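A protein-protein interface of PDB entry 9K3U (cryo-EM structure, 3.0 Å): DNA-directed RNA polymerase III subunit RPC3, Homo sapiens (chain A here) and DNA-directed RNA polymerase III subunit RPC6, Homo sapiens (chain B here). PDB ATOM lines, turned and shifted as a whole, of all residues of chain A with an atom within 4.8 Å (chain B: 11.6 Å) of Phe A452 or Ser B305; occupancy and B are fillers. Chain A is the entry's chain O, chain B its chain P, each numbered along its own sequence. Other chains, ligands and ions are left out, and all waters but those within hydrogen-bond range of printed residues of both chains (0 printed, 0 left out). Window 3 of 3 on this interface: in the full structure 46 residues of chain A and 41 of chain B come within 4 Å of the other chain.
The side-chain carboxylate of Glu A453 lies within salt-bridge range of the guanidinium group of Arg A449 (2.9 Å).
The side-chain hydroxyl (OG) of Ser B303 is in hydrogen-bond range of the side-chain hydroxyl (OG) of Ser B305, at 3.2 Å.
SG of Cys B307 lies close to N of Tyr B309.
SG of Cys B307 lies close to N of Met B310.
Of the printed residues of chain B, Glu A448 touches Pro B304 (3.6 Å).
Arg A449 touches five residues of chain B.
Phe A452 touches one residue of chain B.
No residue of chain B comes within 4 Å of Thr A454.
Lys A455 touches none of the printed residues of chain B.
No residue of chain B comes within 4 Å of Glu A456.
Of chain A, only Arg A449 (3.8 Å) and Phe A452 (3.2 Å) come within 4 Å of Ser B305.
Of the printed residues of chain A, Cys B307 touches Arg A449 (3.7 Å).
Printed residues of chain A within 4 Å of Met B310: Arg A449 (3.6 Å).
Of the printed residues of chain A, Thr B311 touches Arg A449.
Printed residues of chain A within 4 Å of Leu B314: Glu A453.
The nearest residue of chain B that does not touch Phe A452 is Asn B306 (4.9 Å).
The nearest printed residue of chain A that does not touch Ser B305 is Glu A448 (5.2 Å).
The backbone carbonyl oxygen (O) of Pro B304 is in hydrogen-bond range of the guanidinium group (NH1) of Arg A449, 3.2 Å away.
The side-chain hydroxyl (OG1) of Thr B311 sits at hydrogen-bond distance from the guanidinium group (NH2) of Arg A449 (3.1 Å).
Of the 22 printed residues of chain B, 6 touch a printed residue of chain A.
Hydrophobic or aromatic side chains of chain B within 4 Å of the printed part of chain A: Pro B304, Met B310 and Leu B314.
Hydrophobic or aromatic side chains of chain A that line the printed part of chain B: Phe A452.
Among the printed residues, merely in contact across the chains: Glu A448 with Pro B304, Arg A449 with Ser B305, Arg A449 with Cys B307, Arg A449 with Met B310, Phe A452 with Ser B305 and Glu A453 with Leu B314.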
ATOM      1  N   GLU A 448       2.040 -24.544  12.685  1.00  0.00           N
ATOM      2  CA  GLU A 448       1.298 -24.645  13.937  1.00  0.00           C
ATOM      3  C   GLU A 448       2.231 -24.537  15.135  1.00  0.00           C
ATOM      4  O   GLU A 448       1.908 -23.873  16.124  1.00  0.00           O
ATOM      5  CB  GLU A 448       0.519 -25.960  13.978  1.00  0.00           C
ATOM      6  CG  GLU A 448      -0.333 -26.150  15.228  1.00  0.00           C
ATOM      7  CD  GLU A 448      -1.430 -25.111  15.351  1.00  0.00           C
ATOM      8  OE1 GLU A 448      -1.694 -24.398  14.358  1.00  0.00           O
ATOM      9  OE2 GLU A 448      -2.032 -25.008  16.441  1.00  0.00           O
ATOM     10  N   ARG A 449       3.399 -25.179  15.061  1.00  0.00           N
ATOM     11  CA  ARG A 449       4.352 -25.110  16.164  1.00  0.00           C
ATOM     12  C   ARG A 449       4.892 -23.696  16.339  1.00  0.00           C
ATOM     13  O   ARG A 449       5.035 -23.215  17.469  1.00  0.00           O
ATOM     14  CB  ARG A 449       5.494 -26.098  15.930  1.00  0.00           C
ATOM     15  CG  ARG A 449       6.618 -26.028  16.960  1.00  0.00           C
ATOM     16  CD  ARG A 449       6.097 -26.184  18.380  1.00  0.00           C
ATOM     17  NE  ARG A 449       7.180 -26.253  19.356  1.00  0.00           N
ATOM     18  CZ  ARG A 449       7.819 -27.369  19.701  1.00  0.00           C
ATOM     19  NH1 ARG A 449       7.491 -28.530  19.146  1.00  0.00           N
ATOM     20  NH2 ARG A 449       8.792 -27.325  20.600  1.00  0.00           N
ATOM     21  N   ARG A 450       5.203 -23.015  15.233  1.00  0.00           N
ATOM     22  CA  ARG A 450       5.670 -21.637  15.335  1.00  0.00           C
ATOM     23  C   ARG A 450       4.606 -20.747  15.964  1.00  0.00           C
ATOM     24  O   ARG A 450       4.908 -19.928  16.843  1.00  0.00           O
ATOM     25  CB  ARG A 450       6.061 -21.103  13.956  1.00  0.00           C
ATOM     26  CG  ARG A 450       6.828 -19.786  14.007  1.00  0.00           C
ATOM     27  CD  ARG A 450       6.990 -19.153  12.633  1.00  0.00           C
ATOM     28  NE  ARG A 450       5.729 -18.627  12.112  1.00  0.00           N
ATOM     29  CZ  ARG A 450       4.930 -19.265  11.259  1.00  0.00           C
ATOM     30  NH1 ARG A 450       5.246 -20.470  10.804  1.00  0.00           N
ATOM     31  NH2 ARG A 450       3.806 -18.689  10.852  1.00  0.00           N
ATOM     32  N   GLN A 451       3.354 -20.894  15.526  1.00  0.00           N
ATOM     33  CA  GLN A 451       2.276 -20.085  16.089  1.00  0.00           C
ATOM     34  C   GLN A 451       2.076 -20.392  17.567  1.00  0.00           C
ATOM     35  O   GLN A 451       1.838 -19.483  18.368  1.00  0.00           O
ATOM     36  CB  GLN A 451       0.982 -20.324  15.312  1.00  0.00           C
ATOM     37  CG  GLN A 451       1.017 -19.803  13.883  1.00  0.00           C
ATOM     38  CD  GLN A 451      -0.271 -20.073  13.131  1.00  0.00           C
ATOM     39  OE1 GLN A 451      -1.208 -20.663  13.673  1.00  0.00           O
ATOM     40  NE2 GLN A 451      -0.325 -19.646  11.875  1.00  0.00           N
ATOM     41  N   PHE A 452       2.179 -21.666  17.952  1.00  0.00           N
ATOM     42  CA  PHE A 452       2.029 -22.028  19.356  1.00  0.00           C
ATOM     43  C   PHE A 452       3.139 -21.423  20.204  1.00  0.00           C
ATOM     44  O   PHE A 452       2.881 -20.896  21.292  1.00  0.00           O
ATOM     45  CB  PHE A 452       2.010 -23.550  19.505  1.00  0.00           C
ATOM     46  CG  PHE A 452       2.098 -24.020  20.929  1.00  0.00           C
ATOM     47  CD1 PHE A 452       0.974 -24.039  21.739  1.00  0.00           C
ATOM     48  CD2 PHE A 452       3.307 -24.446  21.457  1.00  0.00           C
ATOM     49  CE1 PHE A 452       1.055 -24.470  23.049  1.00  0.00           C
ATOM     50  CE2 PHE A 452       3.393 -24.879  22.766  1.00  0.00           C
ATOM     51  CZ  PHE A 452       2.265 -24.892  23.563  1.00  0.00           C
ATOM     52  N   GLU A 453       4.385 -21.499  19.728  1.00  0.00           N
ATOM     53  CA  GLU A 453       5.487 -20.876  20.452  1.00  0.00           C
ATOM     54  C   GLU A 453       5.276 -19.373  20.597  1.00  0.00           C
ATOM     55  O   GLU A 453       5.446 -18.826  21.696  1.00  0.00           O
ATOM     56  CB  GLU A 453       6.810 -21.159  19.744  1.00  0.00           C
ATOM     57  CG  GLU A 453       7.239 -22.615  19.789  1.00  0.00           C
ATOM     58  CD  GLU A 453       8.549 -22.862  19.066  1.00  0.00           C
ATOM     59  OE1 GLU A 453       9.127 -21.890  18.534  1.00  0.00           O
ATOM     60  OE2 GLU A 453       9.001 -24.026  19.029  1.00  0.00           O
ATOM     61  N   THR A 454       4.906 -18.697  19.508  1.00  0.00           N
ATOM     62  CA  THR A 454       4.682 -17.258  19.576  1.00  0.00           C
ATOM     63  C   THR A 454       3.554 -16.921  20.545  1.00  0.00           C
ATOM     64  O   THR A 454       3.649 -15.949  21.304  1.00  0.00           O
ATOM     65  CB  THR A 454       4.372 -16.709  18.183  1.00  0.00           C
ATOM     66  OG1 THR A 454       5.438 -17.041  17.286  1.00  0.00           O
ATOM     67  CG2 THR A 454       4.205 -15.196  18.229  1.00  0.00           C
ATOM     68  N   LYS A 455       2.484 -17.718  20.547  1.00  0.00           N
ATOM     69  CA  LYS A 455       1.354 -17.437  21.423  1.00  0.00           C
ATOM     70  C   LYS A 455       1.719 -17.658  22.885  1.00  0.00           C
ATOM     71  O   LYS A 455       1.327 -16.869  23.754  1.00  0.00           O
ATOM     72  CB  LYS A 455       0.161 -18.307  21.032  1.00  0.00           C
ATOM     73  CG  LYS A 455      -1.093 -18.055  21.859  1.00  0.00           C
ATOM     74  CD  LYS A 455      -2.285 -18.844  21.335  1.00  0.00           C
ATOM     75  CE  LYS A 455      -2.080 -20.344  21.476  1.00  0.00           C
ATOM     76  NZ  LYS A 455      -3.280 -21.114  21.045  1.00  0.00           N
ATOM     77  N   GLU A 456       2.464 -18.725  23.183  1.00  0.00           N
ATOM     78  CA  GLU A 456       2.824 -19.007  24.566  1.00  0.00           C
ATOM     79  C   GLU A 456       3.893 -18.056  25.091  1.00  0.00           C
ATOM     80  O   GLU A 456       3.964 -17.840  26.304  1.00  0.00           O
ATOM     81  CB  GLU A 456       3.302 -20.454  24.709  1.00  0.00           C
ATOM     82  CG  GLU A 456       4.610 -20.751  23.999  1.00  0.00           C
ATOM     83  CD  GLU A 456       5.029 -22.203  24.135  1.00  0.00           C
ATOM     84  OE1 GLU A 456       4.354 -22.952  24.872  1.00  0.00           O
ATOM     85  OE2 GLU A 456       6.031 -22.594  23.503  1.00  0.00           O
ATOM     86  N   PRO B 286      11.688 -32.704  11.284  1.00  0.00           N
ATOM     87  CA  PRO B 286      11.252 -33.886  12.045  1.00  0.00           C
ATOM     88  C   PRO B 286       9.930 -34.462  11.573  1.00  0.00           C
ATOM     89  O   PRO B 286       9.666 -35.648  11.813  1.00  0.00           O
ATOM     90  CB  PRO B 286      11.149 -33.362  13.483  1.00  0.00           C
ATOM     91  CG  PRO B 286      12.024 -32.160  13.521  1.00  0.00           C
ATOM     92  CD  PRO B 286      11.937 -31.547  12.162  1.00  0.00           C
ATOM     93  N   CYS B 287       9.089 -33.665  10.911  1.00  0.00           N
ATOM     94  CA  CYS B 287       7.787 -34.164  10.477  1.00  0.00           C
ATOM     95  C   CYS B 287       7.921 -35.208   9.379  1.00  0.00           C
ATOM     96  O   CYS B 287       7.133 -36.160   9.333  1.00  0.00           O
ATOM     97  CB  CYS B 287       6.917 -33.004   9.993  1.00  0.00           C
ATOM     98  SG  CYS B 287       6.746 -31.652  11.181  1.00  0.00           S
ATOM     99  N   ASP B 295      -0.702 -40.395  12.980  1.00  0.00           N
ATOM    100  CA  ASP B 295      -1.572 -40.013  14.084  1.00  0.00           C
ATOM    101  C   ASP B 295      -1.452 -38.540  14.460  1.00  0.00           C
ATOM    102  O   ASP B 295      -1.934 -38.150  15.529  1.00  0.00           O
ATOM    103  CB  ASP B 295      -1.271 -40.880  15.309  1.00  0.00           C
ATOM    104  CG  ASP B 295      -1.246 -42.361  14.983  1.00  0.00           C
ATOM    105  OD1 ASP B 295      -1.914 -42.767  14.010  1.00  0.00           O
ATOM    106  OD2 ASP B 295      -0.560 -43.117  15.700  1.00  0.00           O
ATOM    107  N   CYS B 296      -0.828 -37.721  13.619  1.00  0.00           N
ATOM    108  CA  CYS B 296      -0.692 -36.303  13.924  1.00  0.00           C
ATOM    109  C   CYS B 296      -2.051 -35.615  13.884  1.00  0.00           C
ATOM    110  O   CYS B 296      -2.880 -35.888  13.011  1.00  0.00           O
ATOM    111  CB  CYS B 296       0.261 -35.636  12.936  1.00  0.00           C
ATOM    112  SG  CYS B 296       0.370 -33.841  13.110  1.00  0.00           S
ATOM    113  N   HIS B 297      -2.278 -34.716  14.841  1.00  0.00           N
ATOM    114  CA  HIS B 297      -3.531 -33.982  14.911  1.00  0.00           C
ATOM    115  C   HIS B 297      -3.296 -32.685  15.670  1.00  0.00           C
ATOM    116  O   HIS B 297      -2.405 -32.592  16.518  1.00  0.00           O
ATOM    117  CB  HIS B 297      -4.629 -34.810  15.583  1.00  0.00           C
ATOM    118  CG  HIS B 297      -5.996 -34.212  15.463  1.00  0.00           C
ATOM    119  ND1 HIS B 297      -6.527 -33.807  14.258  1.00  0.00           N
ATOM    120  CD2 HIS B 297      -6.942 -33.954  16.395  1.00  0.00           C
ATOM    121  CE1 HIS B 297      -7.741 -33.323  14.452  1.00  0.00           C
ATOM    122  NE2 HIS B 297      -8.017 -33.400  15.743  1.00  0.00           N
ATOM    123  N   GLU B 298      -4.115 -31.682  15.352  1.00  0.00           N
ATOM    124  CA  GLU B 298      -3.998 -30.385  16.011  1.00  0.00           C
ATOM    125  C   GLU B 298      -4.253 -30.510  17.508  1.00  0.00           C
ATOM    126  O   GLU B 298      -3.370 -30.231  18.331  1.00  0.00           O
ATOM    127  CB  GLU B 298      -4.969 -29.389  15.374  1.00  0.00           C
ATOM    128  CG  GLU B 298      -4.904 -27.986  15.964  1.00  0.00           C
ATOM    129  CD  GLU B 298      -5.860 -27.026  15.285  1.00  0.00           C
ATOM    130  OE1 GLU B 298      -6.573 -27.452  14.355  1.00  0.00           O
ATOM    131  OE2 GLU B 298      -5.897 -25.842  15.684  1.00  0.00           O
ATOM    132  N   GLY B 299      -5.460 -30.929  17.880  1.00  0.00           N
ATOM    133  CA  GLY B 299      -5.825 -31.057  19.278  1.00  0.00           C
ATOM    134  C   GLY B 299      -5.893 -32.498  19.744  1.00  0.00           C
ATOM    135  O   GLY B 299      -6.828 -33.225  19.399  1.00  0.00           O
ATOM    136  N   GLY B 300      -4.911 -32.917  20.533  1.00  0.00           N
ATOM    137  CA  GLY B 300      -4.903 -34.277  21.036  1.00  0.00           C
ATOM    138  C   GLY B 300      -3.610 -34.572  21.760  1.00  0.00           C
ATOM    139  O   GLY B 300      -2.864 -33.667  22.138  1.00  0.00           O
ATOM    140  N   GLU B 301      -3.354 -35.869  21.951  1.00  0.00           N
ATOM    141  CA  GLU B 301      -2.134 -36.287  22.634  1.00  0.00           C
ATOM    142  C   GLU B 301      -0.901 -36.000  21.785  1.00  0.00           C
ATOM    143  O   GLU B 301       0.103 -35.486  22.290  1.00  0.00           O
ATOM    144  CB  GLU B 301      -2.212 -37.771  22.982  1.00  0.00           C
ATOM    145  CG  GLU B 301      -3.367 -38.131  23.900  1.00  0.00           C
ATOM    146  CD  GLU B 301      -3.406 -39.609  24.240  1.00  0.00           C
ATOM    147  OE1 GLU B 301      -2.525 -40.353  23.761  1.00  0.00           O
ATOM    148  OE2 GLU B 301      -4.318 -40.025  24.983  1.00  0.00           O
ATOM    149  N   ILE B 302      -0.958 -36.324  20.496  1.00  0.00           N
ATOM    150  CA  ILE B 302       0.144 -36.093  19.569  1.00  0.00           C
ATOM    151  C   ILE B 302      -0.172 -34.799  18.826  1.00  0.00           C
ATOM    152  O   ILE B 302      -0.906 -34.803  17.835  1.00  0.00           O
ATOM    153  CB  ILE B 302       0.338 -37.271  18.612  1.00  0.00           C
ATOM    154  CG1 ILE B 302       0.546 -38.565  19.404  1.00  0.00           C
ATOM    155  CG2 ILE B 302       1.525 -37.016  17.687  1.00  0.00           C
ATOM    156  CD1 ILE B 302       0.686 -39.804  18.544  1.00  0.00           C
ATOM    157  N   SER B 303       0.387 -33.694  19.303  1.00  0.00           N
ATOM    158  CA  SER B 303       0.163 -32.379  18.728  1.00  0.00           C
ATOM    159  C   SER B 303       1.498 -31.703  18.455  1.00  0.00           C
ATOM    160  O   SER B 303       2.452 -31.875  19.220  1.00  0.00           O
ATOM    161  CB  SER B 303      -0.675 -31.500  19.667  1.00  0.00           C
ATOM    162  OG  SER B 303      -0.916 -30.223  19.102  1.00  0.00           O
ATOM    163  N   PRO B 304       1.598 -30.926  17.371  1.00  0.00           N
ATOM    164  CA  PRO B 304       2.869 -30.240  17.086  1.00  0.00           C
ATOM    165  C   PRO B 304       3.274 -29.248  18.160  1.00  0.00           C
ATOM    166  O   PRO B 304       4.470 -28.951  18.286  1.00  0.00           O
ATOM    167  CB  PRO B 304       2.600 -29.541  15.746  1.00  0.00           C
ATOM    168  CG  PRO B 304       1.118 -29.413  15.670  1.00  0.00           C
ATOM    169  CD  PRO B 304       0.573 -30.625  16.358  1.00  0.00           C
ATOM    170  N   SER B 305       2.323 -28.728  18.939  1.00  0.00           N
ATOM    171  CA  SER B 305       2.668 -27.761  19.976  1.00  0.00           C
ATOM    172  C   SER B 305       3.512 -28.398  21.072  1.00  0.00           C
ATOM    173  O   SER B 305       4.496 -27.806  21.528  1.00  0.00           O
ATOM    174  CB  SER B 305       1.394 -27.155  20.566  1.00  0.00           C
ATOM    175  OG  SER B 305       0.556 -28.163  21.107  1.00  0.00           O
ATOM    176  N   ASN B 306       3.147 -29.604  21.505  1.00  0.00           N
ATOM    177  CA  ASN B 306       3.853 -30.317  22.562  1.00  0.00           C
ATOM    178  C   ASN B 306       4.628 -31.516  22.018  1.00  0.00           C
ATOM    179  O   ASN B 306       4.720 -32.556  22.677  1.00  0.00           O
ATOM    180  CB  ASN B 306       2.876 -30.763  23.648  1.00  0.00           C
ATOM    181  CG  ASN B 306       1.742 -31.610  23.104  1.00  0.00           C
ATOM    182  OD1 ASN B 306       1.825 -32.148  21.999  1.00  0.00           O
ATOM    183  ND2 ASN B 306       0.671 -31.735  23.880  1.00  0.00           N
ATOM    184  N   CYS B 307       5.187 -31.386  20.819  1.00  0.00           N
ATOM    185  CA  CYS B 307       5.932 -32.481  20.217  1.00  0.00           C
ATOM    186  C   CYS B 307       7.317 -32.596  20.841  1.00  0.00           C
ATOM    187  O   CYS B 307       7.928 -31.599  21.233  1.00  0.00           O
ATOM    188  CB  CYS B 307       6.058 -32.272  18.709  1.00  0.00           C
ATOM    189  SG  CYS B 307       7.133 -33.470  17.889  1.00  0.00           S
ATOM    190  N   ILE B 308       7.810 -33.831  20.933  1.00  0.00           N
ATOM    191  CA  ILE B 308       9.150 -34.067  21.457  1.00  0.00           C
ATOM    192  C   ILE B 308      10.191 -34.081  20.340  1.00  0.00           C
ATOM    193  O   ILE B 308      11.319 -33.619  20.542  1.00  0.00           O
ATOM    194  CB  ILE B 308       9.187 -35.381  22.256  1.00  0.00           C
ATOM    195  CG1 ILE B 308       8.112 -35.381  23.348  1.00  0.00           C
ATOM    196  CG2 ILE B 308      10.567 -35.597  22.862  1.00  0.00           C
ATOM    197  CD1 ILE B 308       8.234 -34.243  24.348  1.00  0.00           C
ATOM    198  N   TYR B 309       9.837 -34.597  19.162  1.00  0.00           N
ATOM    199  CA  TYR B 309      10.780 -34.620  18.047  1.00  0.00           C
ATOM    200  C   TYR B 309      11.234 -33.209  17.694  1.00  0.00           C
ATOM    201  O   TYR B 309      12.435 -32.919  17.674  1.00  0.00           O
ATOM    202  CB  TYR B 309      10.142 -35.296  16.833  1.00  0.00           C
ATOM    203  CG  TYR B 309       9.715 -36.726  17.076  1.00  0.00           C
ATOM    204  CD1 TYR B 309      10.614 -37.772  16.936  1.00  0.00           C
ATOM    205  CD2 TYR B 309       8.410 -37.026  17.441  1.00  0.00           C
ATOM    206  CE1 TYR B 309      10.227 -39.081  17.154  1.00  0.00           C
ATOM    207  CE2 TYR B 309       8.013 -38.331  17.662  1.00  0.00           C
ATOM    208  CZ  TYR B 309       8.925 -39.355  17.517  1.00  0.00           C
ATOM    209  OH  TYR B 309       8.534 -40.656  17.737  1.00  0.00           O
ATOM    210  N   MET B 310      10.281 -32.319  17.409  1.00  0.00           N
ATOM    211  CA  MET B 310      10.635 -30.945  17.066  1.00  0.00           C
ATOM    212  C   MET B 310      11.287 -30.227  18.239  1.00  0.00           C
ATOM    213  O   MET B 310      12.179 -29.398  18.034  1.00  0.00           O
ATOM    214  CB  MET B 310       9.394 -30.183  16.603  1.00  0.00           C
ATOM    215  CG  MET B 310       8.811 -30.696  15.294  1.00  0.00           C
ATOM    216  SD  MET B 310       7.470 -29.666  14.664  1.00  0.00           S
ATOM    217  CE  MET B 310       6.216 -29.922  15.918  1.00  0.00           C
ATOM    218  N   THR B 311      10.865 -30.529  19.468  1.00  0.00           N
ATOM    219  CA  THR B 311      11.495 -29.915  20.634  1.00  0.00           C
ATOM    220  C   THR B 311      12.984 -30.233  20.674  1.00  0.00           C
ATOM    221  O   THR B 311      13.823 -29.331  20.789  1.00  0.00           O
ATOM    222  CB  THR B 311      10.806 -30.392  21.913  1.00  0.00           C
ATOM    223  OG1 THR B 311       9.408 -30.084  21.850  1.00  0.00           O
ATOM    224  CG2 THR B 311      11.414 -29.720  23.135  1.00  0.00           C
ATOM    225  N   GLU B 312      13.333 -31.519  20.576  1.00  0.00           N
ATOM    226  CA  GLU B 312      14.741 -31.904  20.586  1.00  0.00           C
ATOM    227  C   GLU B 312      15.477 -31.385  19.357  1.00  0.00           C
ATOM    228  O   GLU B 312      16.653 -31.014  19.454  1.00  0.00           O
ATOM    229  CB  GLU B 312      14.866 -33.426  20.671  1.00  0.00           C
ATOM    230  CG  GLU B 312      14.277 -34.026  21.937  1.00  0.00           C
ATOM    231  CD  GLU B 312      14.396 -35.537  21.977  1.00  0.00           C
ATOM    232  OE1 GLU B 312      14.937 -36.116  21.010  1.00  0.00           O
ATOM    233  OE2 GLU B 312      13.949 -36.145  22.971  1.00  0.00           O
ATOM    234  N   TRP B 313      14.810 -31.344  18.202  1.00  0.00           N
ATOM    235  CA  TRP B 313      15.464 -30.869  16.987  1.00  0.00           C
ATOM    236  C   TRP B 313      15.794 -29.385  17.082  1.00  0.00           C
ATOM    237  O   TRP B 313      16.819 -28.935  16.558  1.00  0.00           O
ATOM    238  CB  TRP B 313      14.571 -31.155  15.779  1.00  0.00           C
ATOM    239  CG  TRP B 313      14.986 -30.449  14.528  1.00  0.00           C
ATOM    240  CD1 TRP B 313      16.118 -30.666  13.799  1.00  0.00           C
ATOM    241  CD2 TRP B 313      14.263 -29.417  13.849  1.00  0.00           C
ATOM    242  NE1 TRP B 313      16.148 -29.828  12.710  1.00  0.00           N
ATOM    243  CE2 TRP B 313      15.020 -29.050  12.719  1.00  0.00           C
ATOM    244  CE3 TRP B 313      13.051 -28.763  14.091  1.00  0.00           C
ATOM    245  CZ2 TRP B 313      14.604 -28.063  11.829  1.00  0.00           C
ATOM    246  CZ3 TRP B 313      12.639 -27.781  13.208  1.00  0.00           C
ATOM    247  CH2 TRP B 313      13.413 -27.440  12.091  1.00  0.00           C
ATOM    248  N   LEU B 314      14.935 -28.606  17.747  1.00  0.00           N
ATOM    249  CA  LEU B 314      15.224 -27.193  17.959  1.00  0.00           C
ATOM    250  C   LEU B 314      16.239 -26.987  19.074  1.00  0.00           C
ATOM    251  O   LEU B 314      17.036 -26.042  19.013  1.00  0.00           O
ATOM    252  CB  LEU B 314      13.934 -26.436  18.283  1.00  0.00           C
ATOM    253  CG  LEU B 314      12.875 -26.397  17.179  1.00  0.00           C
ATOM    254  CD1 LEU B 314      11.599 -25.746  17.688  1.00  0.00           C
ATOM    255  CD2 LEU B 314      13.397 -25.666  15.950  1.00  0.00           C
